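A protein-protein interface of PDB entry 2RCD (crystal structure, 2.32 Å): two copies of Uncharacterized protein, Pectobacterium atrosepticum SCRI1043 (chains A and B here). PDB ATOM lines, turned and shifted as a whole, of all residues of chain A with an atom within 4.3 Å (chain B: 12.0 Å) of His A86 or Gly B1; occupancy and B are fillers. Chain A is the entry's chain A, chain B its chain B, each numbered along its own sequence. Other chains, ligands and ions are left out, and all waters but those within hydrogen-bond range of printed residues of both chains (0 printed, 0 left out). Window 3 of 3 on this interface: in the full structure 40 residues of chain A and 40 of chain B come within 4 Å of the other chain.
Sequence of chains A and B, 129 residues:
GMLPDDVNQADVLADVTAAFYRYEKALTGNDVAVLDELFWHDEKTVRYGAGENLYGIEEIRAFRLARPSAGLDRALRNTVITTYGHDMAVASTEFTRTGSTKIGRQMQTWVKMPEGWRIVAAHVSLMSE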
ATOM      1  N   VAL A  12      10.963   9.130   2.219  1.00  0.00           N
ATOM      2  CA  VAL A  12      11.562   7.810   2.498  1.00  0.00           C
ATOM      3  C   VAL A  12      10.433   6.817   2.754  1.00  0.00           C
ATOM      4  O   VAL A  12      10.418   5.734   2.176  1.00  0.00           O
ATOM      5  CB  VAL A  12      12.523   7.809   3.722  1.00  0.00           C
ATOM      6  CG1 VAL A  12      13.147   6.411   3.935  1.00  0.00           C
ATOM      7  CG2 VAL A  12      13.616   8.862   3.557  1.00  0.00           C
ATOM      8  N   TYR A  84      13.902   4.937   9.213  1.00  0.00           N
ATOM      9  CA  TYR A  84      14.991   5.487  10.026  1.00  0.00           C
ATOM     10  C   TYR A  84      16.036   6.114   9.100  1.00  0.00           C
ATOM     11  O   TYR A  84      16.793   5.402   8.429  1.00  0.00           O
ATOM     12  CB  TYR A  84      15.614   4.365  10.879  1.00  0.00           C
ATOM     13  CG  TYR A  84      14.597   3.718  11.777  1.00  0.00           C
ATOM     14  CD1 TYR A  84      14.278   4.291  13.011  1.00  0.00           C
ATOM     15  CD2 TYR A  84      13.926   2.558  11.392  1.00  0.00           C
ATOM     16  CE1 TYR A  84      13.327   3.718  13.845  1.00  0.00           C
ATOM     17  CE2 TYR A  84      12.957   1.991  12.199  1.00  0.00           C
ATOM     18  CZ  TYR A  84      12.666   2.581  13.430  1.00  0.00           C
ATOM     19  OH  TYR A  84      11.727   2.048  14.267  1.00  0.00           O
ATOM     20  N   GLY A  85      16.092   7.438   9.061  1.00  0.00           N
ATOM     21  CA  GLY A  85      17.006   8.105   8.150  1.00  0.00           C
ATOM     22  C   GLY A  85      16.525   7.916   6.713  1.00  0.00           C
ATOM     23  O   GLY A  85      15.314   7.825   6.449  1.00  0.00           O
ATOM     24  N   HIS A  86      17.469   7.800   5.785  1.00  0.00           N
ATOM     25  CA  HIS A  86      17.128   7.720   4.359  1.00  0.00           C
ATOM     26  C   HIS A  86      17.216   6.323   3.741  1.00  0.00           C
ATOM     27  O   HIS A  86      16.866   6.157   2.571  1.00  0.00           O
ATOM     28  CB  HIS A  86      17.961   8.762   3.545  1.00  0.00           C
ATOM     29  CG  HIS A  86      19.451   8.572   3.628  1.00  0.00           C
ATOM     30  ND1 HIS A  86      20.216   9.078   4.659  1.00  0.00           N
ATOM     31  CD2 HIS A  86      20.319   7.948   2.796  1.00  0.00           C
ATOM     32  CE1 HIS A  86      21.484   8.754   4.470  1.00  0.00           C
ATOM     33  NE2 HIS A  86      21.573   8.068   3.346  1.00  0.00           N
ATOM     34  N   ASP A  87      17.614   5.303   4.500  1.00  0.00           N
ATOM     35  CA  ASP A  87      17.822   3.997   3.876  1.00  0.00           C
ATOM     36  C   ASP A  87      17.615   2.738   4.745  1.00  0.00           C
ATOM     37  O   ASP A  87      18.203   1.694   4.489  1.00  0.00           O
ATOM     38  CB  ASP A  87      19.207   4.014   3.200  1.00  0.00           C
ATOM     39  CG  ASP A  87      20.305   4.486   4.127  1.00  0.00           C
ATOM     40  OD1 ASP A  87      20.180   4.251   5.350  1.00  0.00           O
ATOM     41  OD2 ASP A  87      21.289   5.088   3.636  1.00  0.00           O
ATOM     42  N   MET A  88      16.720   2.823   5.720  1.00  0.00           N
ATOM     43  CA  MET A  88      16.450   1.718   6.635  1.00  0.00           C
ATOM     44  C   MET A  88      14.994   1.784   7.060  1.00  0.00           C
ATOM     45  O   MET A  88      14.501   2.852   7.398  1.00  0.00           O
ATOM     46  CB  MET A  88      17.372   1.851   7.842  1.00  0.00           C
ATOM     47  CG  MET A  88      18.865   1.561   7.544  1.00  0.00           C
ATOM     48  SD  MET A  88      20.180   2.346   8.781  1.00  0.00           S
ATOM     49  CE  MET A  88      21.773   1.492   8.053  1.00  0.00           C
ATOM     50  N   LYS A 112      17.827   0.268   1.813  1.00  0.00           N
ATOM     51  CA  LYS A 112      17.937   0.772   0.450  1.00  0.00           C
ATOM     52  C   LYS A 112      19.329   0.473  -0.068  1.00  0.00           C
ATOM     53  O   LYS A 112      20.299   1.045   0.403  1.00  0.00           O
ATOM     54  CB  LYS A 112      17.684   2.277   0.381  1.00  0.00           C
ATOM     55  CG  LYS A 112      17.510   2.831  -1.028  1.00  0.00           C
ATOM     56  CD  LYS A 112      17.397   4.369  -0.998  1.00  0.00           C
ATOM     57  CE  LYS A 112      17.093   4.976  -2.390  1.00  0.00           C
ATOM     58  NZ  LYS A 112      17.256   6.479  -2.430  1.00  0.00           N
ATOM     59  N   TRP A 117      15.196  -0.942  -2.664  1.00  0.00           N
ATOM     60  CA  TRP A 117      14.829  -1.417  -1.325  1.00  0.00           C
ATOM     61  C   TRP A 117      14.835  -2.929  -1.298  1.00  0.00           C
ATOM     62  O   TRP A 117      14.242  -3.573  -2.155  1.00  0.00           O
ATOM     63  CB  TRP A 117      13.457  -0.910  -0.895  1.00  0.00           C
ATOM     64  CG  TRP A 117      13.483   0.517  -0.549  1.00  0.00           C
ATOM     65  CD1 TRP A 117      13.146   1.567  -1.352  1.00  0.00           C
ATOM     66  CD2 TRP A 117      13.910   1.080   0.694  1.00  0.00           C
ATOM     67  NE1 TRP A 117      13.326   2.751  -0.683  1.00  0.00           N
ATOM     68  CE2 TRP A 117      13.795   2.486   0.575  1.00  0.00           C
ATOM     69  CE3 TRP A 117      14.399   0.537   1.886  1.00  0.00           C
ATOM     70  CZ2 TRP A 117      14.139   3.353   1.603  1.00  0.00           C
ATOM     71  CZ3 TRP A 117      14.720   1.398   2.925  1.00  0.00           C
ATOM     72  CH2 TRP A 117      14.586   2.792   2.774  1.00  0.00           C
ATOM     73  N   GLY B   1      21.160   4.820   0.834  1.00  0.00           N
ATOM     74  CA  GLY B   1      22.369   4.258   0.182  1.00  0.00           C
ATOM     75  C   GLY B   1      23.164   3.358   1.092  1.00  0.00           C
ATOM     76  O   GLY B   1      23.651   3.792   2.115  1.00  0.00           O
ATOM     77  N   MET B   2      23.286   2.099   0.694  1.00  0.00           N
ATOM     78  CA  MET B   2      24.026   1.076   1.432  1.00  0.00           C
ATOM     79  C   MET B   2      24.859   0.247   0.435  1.00  0.00           C
ATOM     80  O   MET B   2      24.320  -0.565  -0.311  1.00  0.00           O
ATOM     81  CB  MET B   2      23.049   0.159   2.155  1.00  0.00           C
ATOM     82  CG  MET B   2      23.677  -0.584   3.322  1.00  0.00           C
ATOM     83  SD  MET B   2      24.050   0.701   4.753  1.00  0.00           S
ATOM     84  CE  MET B   2      22.233   1.340   5.088  1.00  0.00           C
ATOM     85  N   LEU B   3      26.166   0.482   0.407  1.00  0.00           N
ATOM     86  CA  LEU B   3      27.052  -0.229  -0.491  1.00  0.00           C
ATOM     87  C   LEU B   3      27.579  -1.465   0.247  1.00  0.00           C
ATOM     88  O   LEU B   3      27.525  -1.517   1.466  1.00  0.00           O
ATOM     89  CB  LEU B   3      28.203   0.680  -0.902  1.00  0.00           C
ATOM     90  CG  LEU B   3      27.828   2.050  -1.452  1.00  0.00           C
ATOM     91  CD1 LEU B   3      29.079   2.787  -1.928  1.00  0.00           C
ATOM     92  CD2 LEU B   3      26.806   1.972  -2.564  1.00  0.00           C
ATOM     93  N   PRO B   4      28.088  -2.468  -0.485  1.00  0.00           N
ATOM     94  CA  PRO B   4      28.627  -3.684   0.119  1.00  0.00           C
ATOM     95  C   PRO B   4      29.696  -3.481   1.194  1.00  0.00           C
ATOM     96  O   PRO B   4      29.797  -4.303   2.115  1.00  0.00           O
ATOM     97  CB  PRO B   4      29.240  -4.419  -1.072  1.00  0.00           C
ATOM     98  CG  PRO B   4      29.390  -3.381  -2.137  1.00  0.00           C
ATOM     99  CD  PRO B   4      28.185  -2.537  -1.951  1.00  0.00           C
ATOM    100  N   ASP B   5      30.484  -2.412   1.090  1.00  0.00           N
ATOM    101  CA  ASP B   5      31.503  -2.109   2.098  1.00  0.00           C
ATOM    102  C   ASP B   5      30.883  -1.574   3.407  1.00  0.00           C
ATOM    103  O   ASP B   5      31.526  -1.615   4.462  1.00  0.00           O
ATOM    104  CB  ASP B   5      32.531  -1.116   1.537  1.00  0.00           C
ATOM    105  N   ASP B   6      29.638  -1.095   3.354  1.00  0.00           N
ATOM    106  CA  ASP B   6      28.955  -0.565   4.536  1.00  0.00           C
ATOM    107  C   ASP B   6      28.386  -1.687   5.428  1.00  0.00           C
ATOM    108  O   ASP B   6      27.834  -1.414   6.489  1.00  0.00           O
ATOM    109  CB  ASP B   6      27.803   0.374   4.131  1.00  0.00           C
ATOM    110  CG  ASP B   6      28.247   1.525   3.215  1.00  0.00           C
ATOM    111  OD1 ASP B   6      29.465   1.756   3.051  1.00  0.00           O
ATOM    112  OD2 ASP B   6      27.362   2.208   2.646  1.00  0.00           O
ATOM    113  N   VAL B   7      28.481  -2.942   4.990  1.00  0.00           N
ATOM    114  CA  VAL B   7      27.966  -4.061   5.773  1.00  0.00           C
ATOM    115  C   VAL B   7      29.070  -4.597   6.683  1.00  0.00           C
ATOM    116  O   VAL B   7      30.212  -4.797   6.263  1.00  0.00           O
ATOM    117  CB  VAL B   7      27.409  -5.179   4.863  1.00  0.00           C
ATOM    118  CG1 VAL B   7      26.838  -6.332   5.697  1.00  0.00           C
ATOM    119  CG2 VAL B   7      26.348  -4.606   3.900  1.00  0.00           C
ATOM    120  N   ASN B   8      28.726  -4.770   7.952  1.00  0.00           N
ATOM    121  CA  ASN B   8      29.628  -5.301   8.968  1.00  0.00           C
ATOM    122  C   ASN B   8      30.958  -4.597   9.140  1.00  0.00           C
ATOM    123  O   ASN B   8      32.023  -5.225   9.086  1.00  0.00           O
ATOM    124  CB  ASN B   8      29.850  -6.800   8.762  1.00  0.00           C
ATOM    125  CG  ASN B   8      28.628  -7.603   9.028  1.00  0.00           C
ATOM    126  OD1 ASN B   8      27.662  -7.120   9.604  1.00  0.00           O
ATOM    127  ND2 ASN B   8      28.658  -8.859   8.605  1.00  0.00           N
ATOM    128  N   GLN B   9      30.897  -3.296   9.388  1.00  0.00           N
ATOM    129  CA  GLN B   9      32.107  -2.557   9.710  1.00  0.00           C
ATOM    130  C   GLN B   9      32.505  -3.039  11.122  1.00  0.00           C
ATOM    131  O   GLN B   9      31.663  -3.113  12.000  1.00  0.00           O
ATOM    132  CB  GLN B   9      31.871  -1.039   9.627  1.00  0.00           C
ATOM    133  CG  GLN B   9      31.651  -0.497   8.183  1.00  0.00           C
ATOM    134  N   THR B  83      25.421  -5.632  10.722  1.00  0.00           N
ATOM    135  CA  THR B  83      25.275  -4.196  10.874  1.00  0.00           C
ATOM    136  C   THR B  83      25.276  -3.575   9.501  1.00  0.00           C
ATOM    137  O   THR B  83      25.900  -4.078   8.569  1.00  0.00           O
ATOM    138  CB  THR B  83      26.380  -3.566  11.737  1.00  0.00           C
ATOM    139  OG1 THR B  83      27.644  -3.702  11.091  1.00  0.00           O
ATOM    140  CG2 THR B  83      26.427  -4.216  13.090  1.00  0.00           C
ATOM    141  N   TYR B  84      24.553  -2.473   9.401  1.00  0.00           N
ATOM    142  CA  TYR B  84      24.369  -1.753   8.161  1.00  0.00           C
ATOM    143  C   TYR B  84      24.810  -0.315   8.416  1.00  0.00           C
ATOM    144  O   TYR B  84      24.197   0.404   9.211  1.00  0.00           O
ATOM    145  CB  TYR B  84      22.908  -1.858   7.771  1.00  0.00           C
ATOM    146  CG  TYR B  84      22.505  -3.293   7.507  1.00  0.00           C
ATOM    147  CD1 TYR B  84      22.844  -3.893   6.314  1.00  0.00           C
ATOM    148  CD2 TYR B  84      21.798  -4.045   8.443  1.00  0.00           C
ATOM    149  CE1 TYR B  84      22.499  -5.174   6.046  1.00  0.00           C
ATOM    150  CE2 TYR B  84      21.460  -5.355   8.187  1.00  0.00           C
ATOM    151  CZ  TYR B  84      21.820  -5.898   6.969  1.00  0.00           C
ATOM    152  OH  TYR B  84      21.519  -7.180   6.615  1.00  0.00           O
ATOM    153  N   GLY B  85      25.909   0.080   7.781  1.00  0.00           N
ATOM    154  CA  GLY B  85      26.491   1.389   8.026  1.00  0.00           C
ATOM    155  C   GLY B  85      26.944   1.438   9.479  1.00  0.00           C
ATOM    156  O   GLY B  85      27.298   0.403  10.071  1.00  0.00           O
ATOM    157  N   HIS B  86      26.873   2.630  10.069  1.00  0.00           N
ATOM    158  CA  HIS B  86      27.299   2.832  11.454  1.00  0.00           C
ATOM    159  C   HIS B  86      26.178   2.848  12.506  1.00  0.00           C
ATOM    160  O   HIS B  86      26.476   2.964  13.696  1.00  0.00           O
ATOM    161  CB  HIS B  86      28.141   4.112  11.571  1.00  0.00           C
ATOM    162  CG  HIS B  86      27.409   5.366  11.208  1.00  0.00           C
ATOM    163  ND1 HIS B  86      27.408   5.879   9.930  1.00  0.00           N
ATOM    164  CD2 HIS B  86      26.678   6.223  11.958  1.00  0.00           C
ATOM    165  CE1 HIS B  86      26.700   6.995   9.905  1.00  0.00           C
ATOM    166  NE2 HIS B  86      26.250   7.228  11.124  1.00  0.00           N
ATOM    167  N   ASP B  87      24.911   2.697  12.120  1.00  0.00           N
ATOM    168  CA  ASP B  87      23.849   2.796  13.124  1.00  0.00           C
ATOM    169  C   ASP B  87      22.578   1.914  12.988  1.00  0.00           C
ATOM    170  O   ASP B  87      21.537   2.252  13.536  1.00  0.00           O
ATOM    171  CB  ASP B  87      23.502   4.281  13.333  1.00  0.00           C
ATOM    172  CG  ASP B  87      23.100   4.975  12.056  1.00  0.00           C
ATOM    173  OD1 ASP B  87      22.716   4.277  11.096  1.00  0.00           O
ATOM    174  OD2 ASP B  87      23.155   6.226  12.017  1.00  0.00           O
ATOM    175  N   MET B  88      22.651   0.798  12.269  1.00  0.00           N
ATOM    176  CA  MET B  88      21.528  -0.146  12.240  1.00  0.00           C
ATOM    177  C   MET B  88      22.082  -1.531  12.199  1.00  0.00           C
ATOM    178  O   MET B  88      23.140  -1.772  11.638  1.00  0.00           O
ATOM    179  CB  MET B  88      20.592   0.017  11.060  1.00  0.00           C
ATOM    180  CG  MET B  88      19.177  -0.737  11.253  1.00  0.00           C
ATOM    181  SD  MET B  88      18.027  -1.050   9.639  1.00  0.00           S
ATOM    182  CE  MET B  88      16.219  -0.269  10.249  1.00  0.00           C
ATOM    183  N   VAL B 111      18.887   0.095  16.312  1.00  0.00           N
ATOM    184  CA  VAL B 111      19.274   1.420  15.820  1.00  0.00           C
ATOM    185  C   VAL B 111      20.126   2.163  16.906  1.00  0.00           C
ATOM    186  O   VAL B 111      19.829   2.109  18.094  1.00  0.00           O
ATOM    187  CB  VAL B 111      18.032   2.205  15.388  1.00  0.00           C
ATOM    188  CG1 VAL B 111      18.394   3.552  14.824  1.00  0.00           C
ATOM    189  CG2 VAL B 111      17.262   1.416  14.311  1.00  0.00           C
ATOM    190  N   LYS B 112      21.217   2.806  16.515  1.00  0.00           N
ATOM    191  CA  LYS B 112      22.023   3.515  17.479  1.00  0.00           C
ATOM    192  C   LYS B 112      21.420   4.901  17.659  1.00  0.00           C
ATOM    193  O   LYS B 112      21.409   5.706  16.738  1.00  0.00           O
ATOM    194  CB  LYS B 112      23.480   3.608  17.040  1.00  0.00           C
ATOM    195  CG  LYS B 112      24.439   4.138  18.126  1.00  0.00           C
ATOM    196  CD  LYS B 112      25.844   4.345  17.562  1.00  0.00           C
ATOM    197  CE  LYS B 112      26.854   4.721  18.659  1.00  0.00           C
ATOM    198  NZ  LYS B 112      28.177   5.272  18.108  1.00  0.00           N
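SD of Met B2 sits at hydrogen-bond distance from N of Gly B85 (3.6 Å).
O of Asp B87 lies within hydrogen-bond range of N of Lys B112, at 3.0 Å.
OD2 of Asp A87 sits at hydrogen-bond distance from NE2 of His A86, at 3.0 Å.
The backbone carbonyl oxygen (O) of Asp A87 is in hydrogen-bond range of the backbone NH (N) of Lys A112, at 3.1 Å.
A ring nitrogen (NE2) of His B86 is in hydrogen-bond range of the side-chain carboxylate (OD2) of Asp B87 (3.4 Å).
Tyr A84 touches Met B88 (CD2 to CE, 3.8 Å).
CD2 of His A86 touches N of Gly B1 (3.8 Å).
Asp A87 touches Met B2 (OD1 to CE, 3.6 Å).
Met B2 touches Met A88.
O of Tyr B84 touches CE of Met A88 (2.9 Å).
Met A88 touches Asp B87.
Met B88 touches Met A88 (CB to SD, 3.3 Å).
Lys A112 touches Gly B1.
Tyr A84 touches Met B88, and with the chains exchanged Met A88 touches Tyr B84.
Met A88 touches Asp B87, but with the chains exchanged Asp A87 does not touch Met B88 (5.8 Å).
Met B88 touches its own counterpart, Met A88.
6 positions are printed for both chains.
Of the 10 pairs that touch across the chains among the printed residues, 3 have their exchanged pair printed and touching as well.
O of Lys A112 lies within hydrogen-bond range of N of Met B2 (3.2 Å).
The backbone NH (N) of Gly B1 sits at hydrogen-bond distance from the side-chain carboxylate (OD2) of Asp A87 (2.8 Å).
No residue of chain B comes within 4 Å of Val A12.
Of the printed residues of chain B, Tyr A84 touches Met B88 (3.8 Å).
No residue of chain B comes within 4 Å of Gly A85.
Of chain B, only Gly B1 (3.8 Å) comes within 4 Å of His A86.
Of chain B, only Gly B1 and Met B2 come within 4 Å of Asp A87.
Of the printed residues of chain A, Gly B1 touches His A86, Asp A87 and Lys A112.
Printed residues of chain A within 4 Å of Met B2: Asp A87, Met A88 and Lys A112.
Printed residues of chain A within 4 Å of Asp B87: Met A88.
The nearest residue of chain B that does not touch His A86 is Met B2 (6.8 Å).
The nearest printed residue of chain A that does not touch Gly B1 is Met A88 (6.6 Å).
Hydrophobic or aromatic side chains of chain B within 4 Å of the printed part of chain A: Met B2, Tyr B84 and Met B88.
Printed residues of chain A that touch a printed residue of chain B: Tyr A84, His A86, Asp A87, Met A88 and Lys A112.
Hydrophobic or aromatic side chains of chain A within 4 Å of the printed part of chain B: Tyr A84, His A86 and Met A88.
Among the printed residues, 10 pairs touch across the chains.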
